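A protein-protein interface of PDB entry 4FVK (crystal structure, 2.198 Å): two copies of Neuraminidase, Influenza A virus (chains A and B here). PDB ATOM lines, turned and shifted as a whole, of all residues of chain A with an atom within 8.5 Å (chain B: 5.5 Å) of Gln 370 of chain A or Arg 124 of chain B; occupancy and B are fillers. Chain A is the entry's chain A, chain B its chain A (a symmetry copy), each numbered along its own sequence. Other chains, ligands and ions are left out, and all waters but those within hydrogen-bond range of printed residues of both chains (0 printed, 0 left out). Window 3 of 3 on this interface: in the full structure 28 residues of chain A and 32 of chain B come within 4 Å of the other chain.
Gln 370 of chain A touches four residues of chain B.
Of the printed residues of chain A, Ser 141 of chain B touches Gln 370 (3.0 Å).
Printed residues of chain B within 4 Å of Val 25 of chain A: Phe 127.
Gly 146 of chain B touches none of the printed residues of chain A.
The nearest residue of chain B that does not touch Gln 370 of chain A is Phe 127 of chain B (4.1 Å).
The nearest residue of chain A that does not touch Arg 124 of chain B is Asn 371 of chain A (7.6 Å).
The nearest printed residue of chain B that does not touch Val 25 of chain A is Ser 141 of chain B (9.1 Å).
Of the 17 printed residues of chain A, 4 touch a printed residue of chain B.
Printed residues of chain A that touch a printed residue of chain B: Val 25, Val 369, Gln 370 and Trp 374.
Among the printed residues, no Asp or Glu carboxylate lies within 4 Å of a Lys or Arg side-chain nitrogen of the other chain.
No position is printed for both chains.
Of the 7 pairs that touch across the chains among the printed residues, none has its exchanged pair printed and touching as well.
OH of Tyr 313 of chain A lies close to O of Val 369 of chain A (3.2 Å).
The backbone NH (N) of Trp 374 of chain A is in hydrogen-bond range of the backbone carbonyl oxygen (O) of Leu 315 of chain A (2.7 Å).
The backbone NH (N) of Arg 124 of chain B lies within hydrogen-bond range of the backbone carbonyl oxygen (O) of Gly 145 of chain B, at 3.3 Å.
The backbone carbonyl oxygen of Ser 126 of chain B sits at hydrogen-bond distance from the backbone NH of Ala 142 of chain B (3.2 Å).
The side-chain amide oxygen (OE1) of Gln 370 of chain A lies within hydrogen-bond range of the side-chain hydroxyl (OG) of Ser 141 of chain B, at 3.0 Å.
Among the printed residues, pairs that only touch across the chains: Gln 370 of chain A with Asn 125 of chain B (3.5 Å), Gln 370 of chain A with Ser 126 of chain B (3.8 Å), Val 25 of chain A with Phe 127 of chain B (3.8 Å), Gln 370 of chain A with Arg 124 of chain B (3.8 Å), Trp 374 of chain A with Phe 127 of chain B (3.9 Å) and Val 369 of chain A with Phe 127 of chain B (3.95 Å).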
ATOM      1  N   LYS A  22     -17.474  16.021 -28.100  1.00  0.00           N
ATOM      2  CA  LYS A  22     -18.839  16.002 -27.588  1.00  0.00           C
ATOM      3  C   LYS A  22     -19.635  17.219 -28.052  1.00  0.00           C
ATOM      4  O   LYS A  22     -20.812  17.360 -27.719  1.00  0.00           O
ATOM      5  CB  LYS A  22     -18.839  15.930 -26.055  1.00  0.00           C
ATOM      6  CG  LYS A  22     -18.055  14.750 -25.485  1.00  0.00           C
ATOM      7  CD  LYS A  22     -18.927  13.542 -25.233  1.00  0.00           C
ATOM      8  CE  LYS A  22     -18.224  12.561 -24.309  1.00  0.00           C
ATOM      9  NZ  LYS A  22     -19.077  11.358 -24.085  1.00  0.00           N
ATOM     10  N   GLY A  23     -18.991  18.101 -28.812  1.00  0.00           N
ATOM     11  CA  GLY A  23     -19.682  19.232 -29.399  1.00  0.00           C
ATOM     12  C   GLY A  23     -18.768  20.094 -30.262  1.00  0.00           C
ATOM     13  O   GLY A  23     -17.575  19.802 -30.414  1.00  0.00           O
ATOM     14  N   TRP A  24     -19.332  21.154 -30.832  1.00  0.00           N
ATOM     15  CA  TRP A  24     -18.601  22.000 -31.790  1.00  0.00           C
ATOM     16  C   TRP A  24     -18.852  23.466 -31.494  1.00  0.00           C
ATOM     17  O   TRP A  24     -19.997  23.890 -31.412  1.00  0.00           O
ATOM     18  CB  TRP A  24     -19.062  21.699 -33.211  1.00  0.00           C
ATOM     19  CG  TRP A  24     -18.960  20.251 -33.550  1.00  0.00           C
ATOM     20  CD1 TRP A  24     -19.878  19.267 -33.273  1.00  0.00           C
ATOM     21  CD2 TRP A  24     -17.863  19.611 -34.200  1.00  0.00           C
ATOM     22  NE1 TRP A  24     -19.421  18.059 -33.732  1.00  0.00           N
ATOM     23  CE2 TRP A  24     -18.186  18.241 -34.306  1.00  0.00           C
ATOM     24  CE3 TRP A  24     -16.649  20.065 -34.722  1.00  0.00           C
ATOM     25  CZ2 TRP A  24     -17.333  17.322 -34.909  1.00  0.00           C
ATOM     26  CZ3 TRP A  24     -15.801  19.148 -35.324  1.00  0.00           C
ATOM     27  CH2 TRP A  24     -16.143  17.793 -35.402  1.00  0.00           C
ATOM     28  N   VAL A  25     -17.786  24.234 -31.306  1.00  0.00           N
ATOM     29  CA  VAL A  25     -17.923  25.661 -31.058  1.00  0.00           C
ATOM     30  C   VAL A  25     -17.283  26.443 -32.198  1.00  0.00           C
ATOM     31  O   VAL A  25     -16.271  26.028 -32.744  1.00  0.00           O
ATOM     32  CB  VAL A  25     -17.263  26.075 -29.721  1.00  0.00           C
ATOM     33  CG1 VAL A  25     -18.029  25.491 -28.541  1.00  0.00           C
ATOM     34  CG2 VAL A  25     -15.795  25.638 -29.694  1.00  0.00           C
ATOM     35  N   SER A 312     -27.041  15.549 -31.086  1.00  0.00           N
ATOM     36  CA  SER A 312     -27.509  16.184 -32.307  1.00  0.00           C
ATOM     37  C   SER A 312     -27.591  17.693 -32.154  1.00  0.00           C
ATOM     38  O   SER A 312     -28.451  18.196 -31.444  1.00  0.00           O
ATOM     39  CB  SER A 312     -28.874  15.652 -32.698  1.00  0.00           C
ATOM     40  OG  SER A 312     -29.331  16.296 -33.875  1.00  0.00           O
ATOM     41  N   TYR A 313     -26.711  18.415 -32.845  1.00  0.00           N
ATOM     42  CA  TYR A 313     -26.623  19.860 -32.675  1.00  0.00           C
ATOM     43  C   TYR A 313     -27.057  20.618 -33.909  1.00  0.00           C
ATOM     44  O   TYR A 313     -26.535  20.411 -34.990  1.00  0.00           O
ATOM     45  CB  TYR A 313     -25.205  20.268 -32.332  1.00  0.00           C
ATOM     46  CG  TYR A 313     -24.737  19.886 -30.956  1.00  0.00           C
ATOM     47  CD1 TYR A 313     -23.870  18.817 -30.773  1.00  0.00           C
ATOM     48  CD2 TYR A 313     -25.127  20.616 -29.842  1.00  0.00           C
ATOM     49  CE1 TYR A 313     -23.407  18.475 -29.521  1.00  0.00           C
ATOM     50  CE2 TYR A 313     -24.675  20.273 -28.578  1.00  0.00           C
ATOM     51  CZ  TYR A 313     -23.810  19.207 -28.426  1.00  0.00           C
ATOM     52  OH  TYR A 313     -23.350  18.854 -27.176  1.00  0.00           O
ATOM     53  N   GLU A 314     -28.006  21.523 -33.739  1.00  0.00           N
ATOM     54  CA  GLU A 314     -28.459  22.327 -34.856  1.00  0.00           C
ATOM     55  C   GLU A 314     -27.710  23.662 -34.812  1.00  0.00           C
ATOM     56  O   GLU A 314     -28.190  24.626 -34.226  1.00  0.00           O
ATOM     57  CB  GLU A 314     -29.972  22.523 -34.758  1.00  0.00           C
ATOM     58  CG  GLU A 314     -30.653  22.910 -36.055  1.00  0.00           C
ATOM     59  CD  GLU A 314     -32.160  23.019 -35.899  1.00  0.00           C
ATOM     60  OE1 GLU A 314     -32.695  24.140 -36.014  1.00  0.00           O
ATOM     61  OE2 GLU A 314     -32.809  21.982 -35.649  1.00  0.00           O
ATOM     62  N   LEU A 315     -26.510  23.699 -35.394  1.00  0.00           N
ATOM     63  CA  LEU A 315     -25.641  24.880 -35.299  1.00  0.00           C
ATOM     64  C   LEU A 315     -26.205  26.082 -36.060  1.00  0.00           C
ATOM     65  O   LEU A 315     -26.093  27.213 -35.606  1.00  0.00           O
ATOM     66  CB  LEU A 315     -24.229  24.567 -35.795  1.00  0.00           C
ATOM     67  CG  LEU A 315     -23.455  23.498 -35.020  1.00  0.00           C
ATOM     68  CD1 LEU A 315     -22.117  23.248 -35.697  1.00  0.00           C
ATOM     69  CD2 LEU A 315     -23.258  23.902 -33.586  1.00  0.00           C
ATOM     70  N   ILE A 365     -14.927  20.032 -29.318  1.00  0.00           N
ATOM     71  CA  ILE A 365     -14.438  20.056 -27.933  1.00  0.00           C
ATOM     72  C   ILE A 365     -14.942  18.827 -27.176  1.00  0.00           C
ATOM     73  O   ILE A 365     -15.974  18.268 -27.535  1.00  0.00           O
ATOM     74  CB  ILE A 365     -14.787  21.373 -27.161  1.00  0.00           C
ATOM     75  CG1 ILE A 365     -16.241  21.384 -26.686  1.00  0.00           C
ATOM     76  CG2 ILE A 365     -14.431  22.640 -27.975  1.00  0.00           C
ATOM     77  CD1 ILE A 365     -17.245  21.651 -27.739  1.00  0.00           C
ATOM     78  N   SER A 367     -15.930  18.690 -24.044  1.00  0.00           N
ATOM     79  CA  SER A 367     -16.921  19.051 -23.036  1.00  0.00           C
ATOM     80  C   SER A 367     -18.266  19.282 -23.776  1.00  0.00           C
ATOM     81  O   SER A 367     -18.276  19.745 -24.915  1.00  0.00           O
ATOM     82  CB  SER A 367     -16.418  20.279 -22.221  1.00  0.00           C
ATOM     83  OG  SER A 367     -14.971  20.282 -22.005  1.00  0.00           O
ATOM     84  N   PRO A 368     -19.407  18.899 -23.176  1.00  0.00           N
ATOM     85  CA  PRO A 368     -20.676  19.137 -23.889  1.00  0.00           C
ATOM     86  C   PRO A 368     -21.143  20.606 -23.808  1.00  0.00           C
ATOM     87  O   PRO A 368     -20.549  21.407 -23.078  1.00  0.00           O
ATOM     88  CB  PRO A 368     -21.670  18.213 -23.168  1.00  0.00           C
ATOM     89  CG  PRO A 368     -20.831  17.288 -22.326  1.00  0.00           C
ATOM     90  CD  PRO A 368     -19.606  18.076 -21.974  1.00  0.00           C
ATOM     91  N   VAL A 369     -22.195  20.949 -24.550  1.00  0.00           N
ATOM     92  CA  VAL A 369     -22.628  22.344 -24.665  1.00  0.00           C
ATOM     93  C   VAL A 369     -24.063  22.428 -25.206  1.00  0.00           C
ATOM     94  O   VAL A 369     -24.571  21.466 -25.785  1.00  0.00           O
ATOM     95  CB  VAL A 369     -21.633  23.153 -25.550  1.00  0.00           C
ATOM     96  CG1 VAL A 369     -21.539  22.552 -26.962  1.00  0.00           C
ATOM     97  CG2 VAL A 369     -21.986  24.634 -25.601  1.00  0.00           C
ATOM     98  N   GLN A 370     -24.720  23.567 -24.996  1.00  0.00           N
ATOM     99  CA  GLN A 370     -26.108  23.760 -25.404  1.00  0.00           C
ATOM    100  C   GLN A 370     -26.279  23.872 -26.905  1.00  0.00           C
ATOM    101  O   GLN A 370     -25.354  24.228 -27.622  1.00  0.00           O
ATOM    102  CB  GLN A 370     -26.721  25.003 -24.745  1.00  0.00           C
ATOM    103  CG  GLN A 370     -26.925  24.891 -23.251  1.00  0.00           C
ATOM    104  CD  GLN A 370     -25.612  24.805 -22.507  1.00  0.00           C
ATOM    105  OE1 GLN A 370     -24.753  25.691 -22.625  1.00  0.00           O
ATOM    106  NE2 GLN A 370     -25.431  23.716 -21.757  1.00  0.00           N
ATOM    107  N   ASN A 371     -27.495  23.590 -27.349  1.00  0.00           N
ATOM    108  CA  ASN A 371     -27.870  23.568 -28.748  1.00  0.00           C
ATOM    109  C   ASN A 371     -28.140  24.976 -29.265  1.00  0.00           C
ATOM    110  O   ASN A 371     -29.212  25.260 -29.814  1.00  0.00           O
ATOM    111  CB  ASN A 371     -29.113  22.685 -28.915  1.00  0.00           C
ATOM    112  CG  ASN A 371     -29.393  22.330 -30.360  1.00  0.00           C
ATOM    113  OD1 ASN A 371     -28.506  22.393 -31.206  1.00  0.00           O
ATOM    114  ND2 ASN A 371     -30.636  21.959 -30.652  1.00  0.00           N
ATOM    115  N   ILE A 372     -27.158  25.856 -29.104  1.00  0.00           N
ATOM    116  CA  ILE A 372     -27.309  27.239 -29.544  1.00  0.00           C
ATOM    117  C   ILE A 372     -27.416  27.341 -31.062  1.00  0.00           C
ATOM    118  O   ILE A 372     -26.742  26.626 -31.797  1.00  0.00           O
ATOM    119  CB  ILE A 372     -26.205  28.166 -28.960  1.00  0.00           C
ATOM    120  CG1 ILE A 372     -25.651  29.104 -30.031  1.00  0.00           C
ATOM    121  CG2 ILE A 372     -25.104  27.360 -28.308  1.00  0.00           C
ATOM    122  CD1 ILE A 372     -26.220  30.500 -29.963  1.00  0.00           C
ATOM    123  N   ASN A 373     -28.334  28.186 -31.513  1.00  0.00           N
ATOM    124  CA  ASN A 373     -28.519  28.473 -32.917  1.00  0.00           C
ATOM    125  C   ASN A 373     -27.603  29.643 -33.269  1.00  0.00           C
ATOM    126  O   ASN A 373     -27.678  30.693 -32.623  1.00  0.00           O
ATOM    127  CB  ASN A 373     -29.979  28.852 -33.175  1.00  0.00           C
ATOM    128  CG  ASN A 373     -30.234  29.261 -34.620  1.00  0.00           C
ATOM    129  OD1 ASN A 373     -29.328  29.231 -35.452  1.00  0.00           O
ATOM    130  ND2 ASN A 373     -31.475  29.636 -34.926  1.00  0.00           N
ATOM    131  N   TRP A 374     -26.739  29.471 -34.273  1.00  0.00           N
ATOM    132  CA  TRP A 374     -25.781  30.536 -34.644  1.00  0.00           C
ATOM    133  C   TRP A 374     -26.250  31.486 -35.750  1.00  0.00           C
ATOM    134  O   TRP A 374     -25.467  32.310 -36.204  1.00  0.00           O
ATOM    135  CB  TRP A 374     -24.374  29.988 -34.967  1.00  0.00           C
ATOM    136  CG  TRP A 374     -23.745  29.324 -33.797  1.00  0.00           C
ATOM    137  CD1 TRP A 374     -23.724  27.983 -33.534  1.00  0.00           C
ATOM    138  CD2 TRP A 374     -23.090  29.955 -32.694  1.00  0.00           C
ATOM    139  NE1 TRP A 374     -23.099  27.738 -32.348  1.00  0.00           N
ATOM    140  CE2 TRP A 374     -22.695  28.930 -31.805  1.00  0.00           C
ATOM    141  CE3 TRP A 374     -22.783  31.289 -32.377  1.00  0.00           C
ATOM    142  CZ2 TRP A 374     -22.021  29.187 -30.619  1.00  0.00           C
ATOM    143  CZ3 TRP A 374     -22.101  31.545 -31.192  1.00  0.00           C
ATOM    144  CH2 TRP A 374     -21.722  30.496 -30.333  1.00  0.00           C
ATOM    145  N   ARG B 122     -27.949  33.986 -25.161  1.00  0.00           N
ATOM    146  CA  ARG B 122     -28.726  35.034 -24.515  1.00  0.00           C
ATOM    147  C   ARG B 122     -29.288  34.674 -23.139  1.00  0.00           C
ATOM    148  O   ARG B 122     -29.436  35.556 -22.290  1.00  0.00           O
ATOM    149  CB  ARG B 122     -29.833  35.540 -25.444  1.00  0.00           C
ATOM    150  CG  ARG B 122     -29.546  36.908 -26.051  1.00  0.00           C
ATOM    151  CD  ARG B 122     -30.741  37.398 -26.842  1.00  0.00           C
ATOM    152  NE  ARG B 122     -31.978  37.205 -26.088  1.00  0.00           N
ATOM    153  CZ  ARG B 122     -33.183  37.576 -26.508  1.00  0.00           C
ATOM    154  NH1 ARG B 122     -33.329  38.172 -27.684  1.00  0.00           N
ATOM    155  NH2 ARG B 122     -34.245  37.352 -25.744  1.00  0.00           N
ATOM    156  N   ASP B 123     -29.601  33.398 -22.916  1.00  0.00           N
ATOM    157  CA  ASP B 123     -30.160  32.976 -21.629  1.00  0.00           C
ATOM    158  C   ASP B 123     -29.552  31.671 -21.128  1.00  0.00           C
ATOM    159  O   ASP B 123     -28.368  31.604 -20.805  1.00  0.00           O
ATOM    160  CB  ASP B 123     -31.677  32.809 -21.721  1.00  0.00           C
ATOM    161  CG  ASP B 123     -32.334  33.863 -22.592  1.00  0.00           C
ATOM    162  OD1 ASP B 123     -32.484  35.017 -22.128  1.00  0.00           O
ATOM    163  OD2 ASP B 123     -32.715  33.526 -23.737  1.00  0.00           O
ATOM    164  N   ARG B 124     -30.377  30.632 -21.050  1.00  0.00           N
ATOM    165  CA  ARG B 124     -29.914  29.350 -20.533  1.00  0.00           C
ATOM    166  C   ARG B 124     -28.945  28.644 -21.479  1.00  0.00           C
ATOM    167  O   ARG B 124     -28.177  27.788 -21.057  1.00  0.00           O
ATOM    168  CB  ARG B 124     -31.089  28.441 -20.159  1.00  0.00           C
ATOM    169  CG  ARG B 124     -32.309  28.571 -21.058  1.00  0.00           C
ATOM    170  CD  ARG B 124     -33.544  27.983 -20.378  1.00  0.00           C
ATOM    171  NE  ARG B 124     -33.958  26.709 -20.960  1.00  0.00           N
ATOM    172  CZ  ARG B 124     -35.062  26.537 -21.682  1.00  0.00           C
ATOM    173  NH1 ARG B 124     -35.876  27.560 -21.909  1.00  0.00           N
ATOM    174  NH2 ARG B 124     -35.356  25.340 -22.172  1.00  0.00           N
ATOM    175  N   ASN B 125     -28.971  29.011 -22.754  1.00  0.00           N
ATOM    176  CA  ASN B 125     -28.001  28.474 -23.701  1.00  0.00           C
ATOM    177  C   ASN B 125     -26.612  29.100 -23.574  1.00  0.00           C
ATOM    178  O   ASN B 125     -25.681  28.681 -24.257  1.00  0.00           O
ATOM    179  CB  ASN B 125     -28.482  28.662 -25.138  1.00  0.00           C
ATOM    180  CG  ASN B 125     -29.658  27.787 -25.478  1.00  0.00           C
ATOM    181  OD1 ASN B 125     -30.038  26.905 -24.708  1.00  0.00           O
ATOM    182  ND2 ASN B 125     -30.242  28.021 -26.650  1.00  0.00           N
ATOM    183  N   SER B 126     -26.481  30.106 -22.716  1.00  0.00           N
ATOM    184  CA  SER B 126     -25.255  30.886 -22.636  1.00  0.00           C
ATOM    185  C   SER B 126     -24.061  30.060 -22.174  1.00  0.00           C
ATOM    186  O   SER B 126     -24.197  29.188 -21.312  1.00  0.00           O
ATOM    187  CB  SER B 126     -25.451  32.102 -21.734  1.00  0.00           C
ATOM    188  OG  SER B 126     -24.211  32.660 -21.369  1.00  0.00           O
ATOM    189  N   PHE B 127     -22.887  30.333 -22.755  1.00  0.00           N
ATOM    190  CA  PHE B 127     -21.677  29.623 -22.349  1.00  0.00           C
ATOM    191  C   PHE B 127     -20.397  30.430 -22.606  1.00  0.00           C
ATOM    192  O   PHE B 127     -20.374  31.363 -23.412  1.00  0.00           O
ATOM    193  CB  PHE B 127     -21.592  28.245 -23.034  1.00  0.00           C
ATOM    194  CG  PHE B 127     -21.081  28.307 -24.451  1.00  0.00           C
ATOM    195  CD1 PHE B 127     -19.768  27.982 -24.747  1.00  0.00           C
ATOM    196  CD2 PHE B 127     -21.912  28.716 -25.485  1.00  0.00           C
ATOM    197  CE1 PHE B 127     -19.295  28.049 -26.052  1.00  0.00           C
ATOM    198  CE2 PHE B 127     -21.449  28.776 -26.791  1.00  0.00           C
ATOM    199  CZ  PHE B 127     -20.139  28.454 -27.074  1.00  0.00           C
ATOM    200  N   SER B 141     -20.650  26.234 -18.985  1.00  0.00           N
ATOM    201  CA  SER B 141     -22.013  26.709 -19.221  1.00  0.00           C
ATOM    202  C   SER B 141     -22.579  27.537 -18.063  1.00  0.00           C
ATOM    203  O   SER B 141     -22.025  27.557 -16.971  1.00  0.00           O
ATOM    204  CB  SER B 141     -22.943  25.521 -19.508  1.00  0.00           C
ATOM    205  OG  SER B 141     -22.577  24.865 -20.713  1.00  0.00           O
ATOM    206  N   ALA B 142     -23.675  28.237 -18.333  1.00  0.00           N
ATOM    207  CA  ALA B 142     -24.419  28.956 -17.305  1.00  0.00           C
ATOM    208  C   ALA B 142     -24.941  27.965 -16.277  1.00  0.00           C
ATOM    209  O   ALA B 142     -25.366  26.869 -16.636  1.00  0.00           O
ATOM    210  CB  ALA B 142     -25.574  29.709 -17.934  1.00  0.00           C
ATOM    211  N   GLY B 145     -29.148  30.038 -14.843  1.00  0.00           N
ATOM    212  CA  GLY B 145     -30.120  30.556 -15.787  1.00  0.00           C
ATOM    213  C   GLY B 145     -29.516  31.411 -16.888  1.00  0.00           C
ATOM    214  O   GLY B 145     -30.168  31.698 -17.893  1.00  0.00           O
ATOM    215  N   GLY B 146     -28.271  31.836 -16.698  1.00  0.00           N
ATOM    216  CA  GLY B 146     -27.634  32.723 -17.652  1.00  0.00           C
ATOM    217  C   GLY B 146     -28.315  34.071 -17.751  1.00  0.00           C
ATOM    218  O   GLY B 146     -29.279  34.339 -17.028  1.00  0.00           O
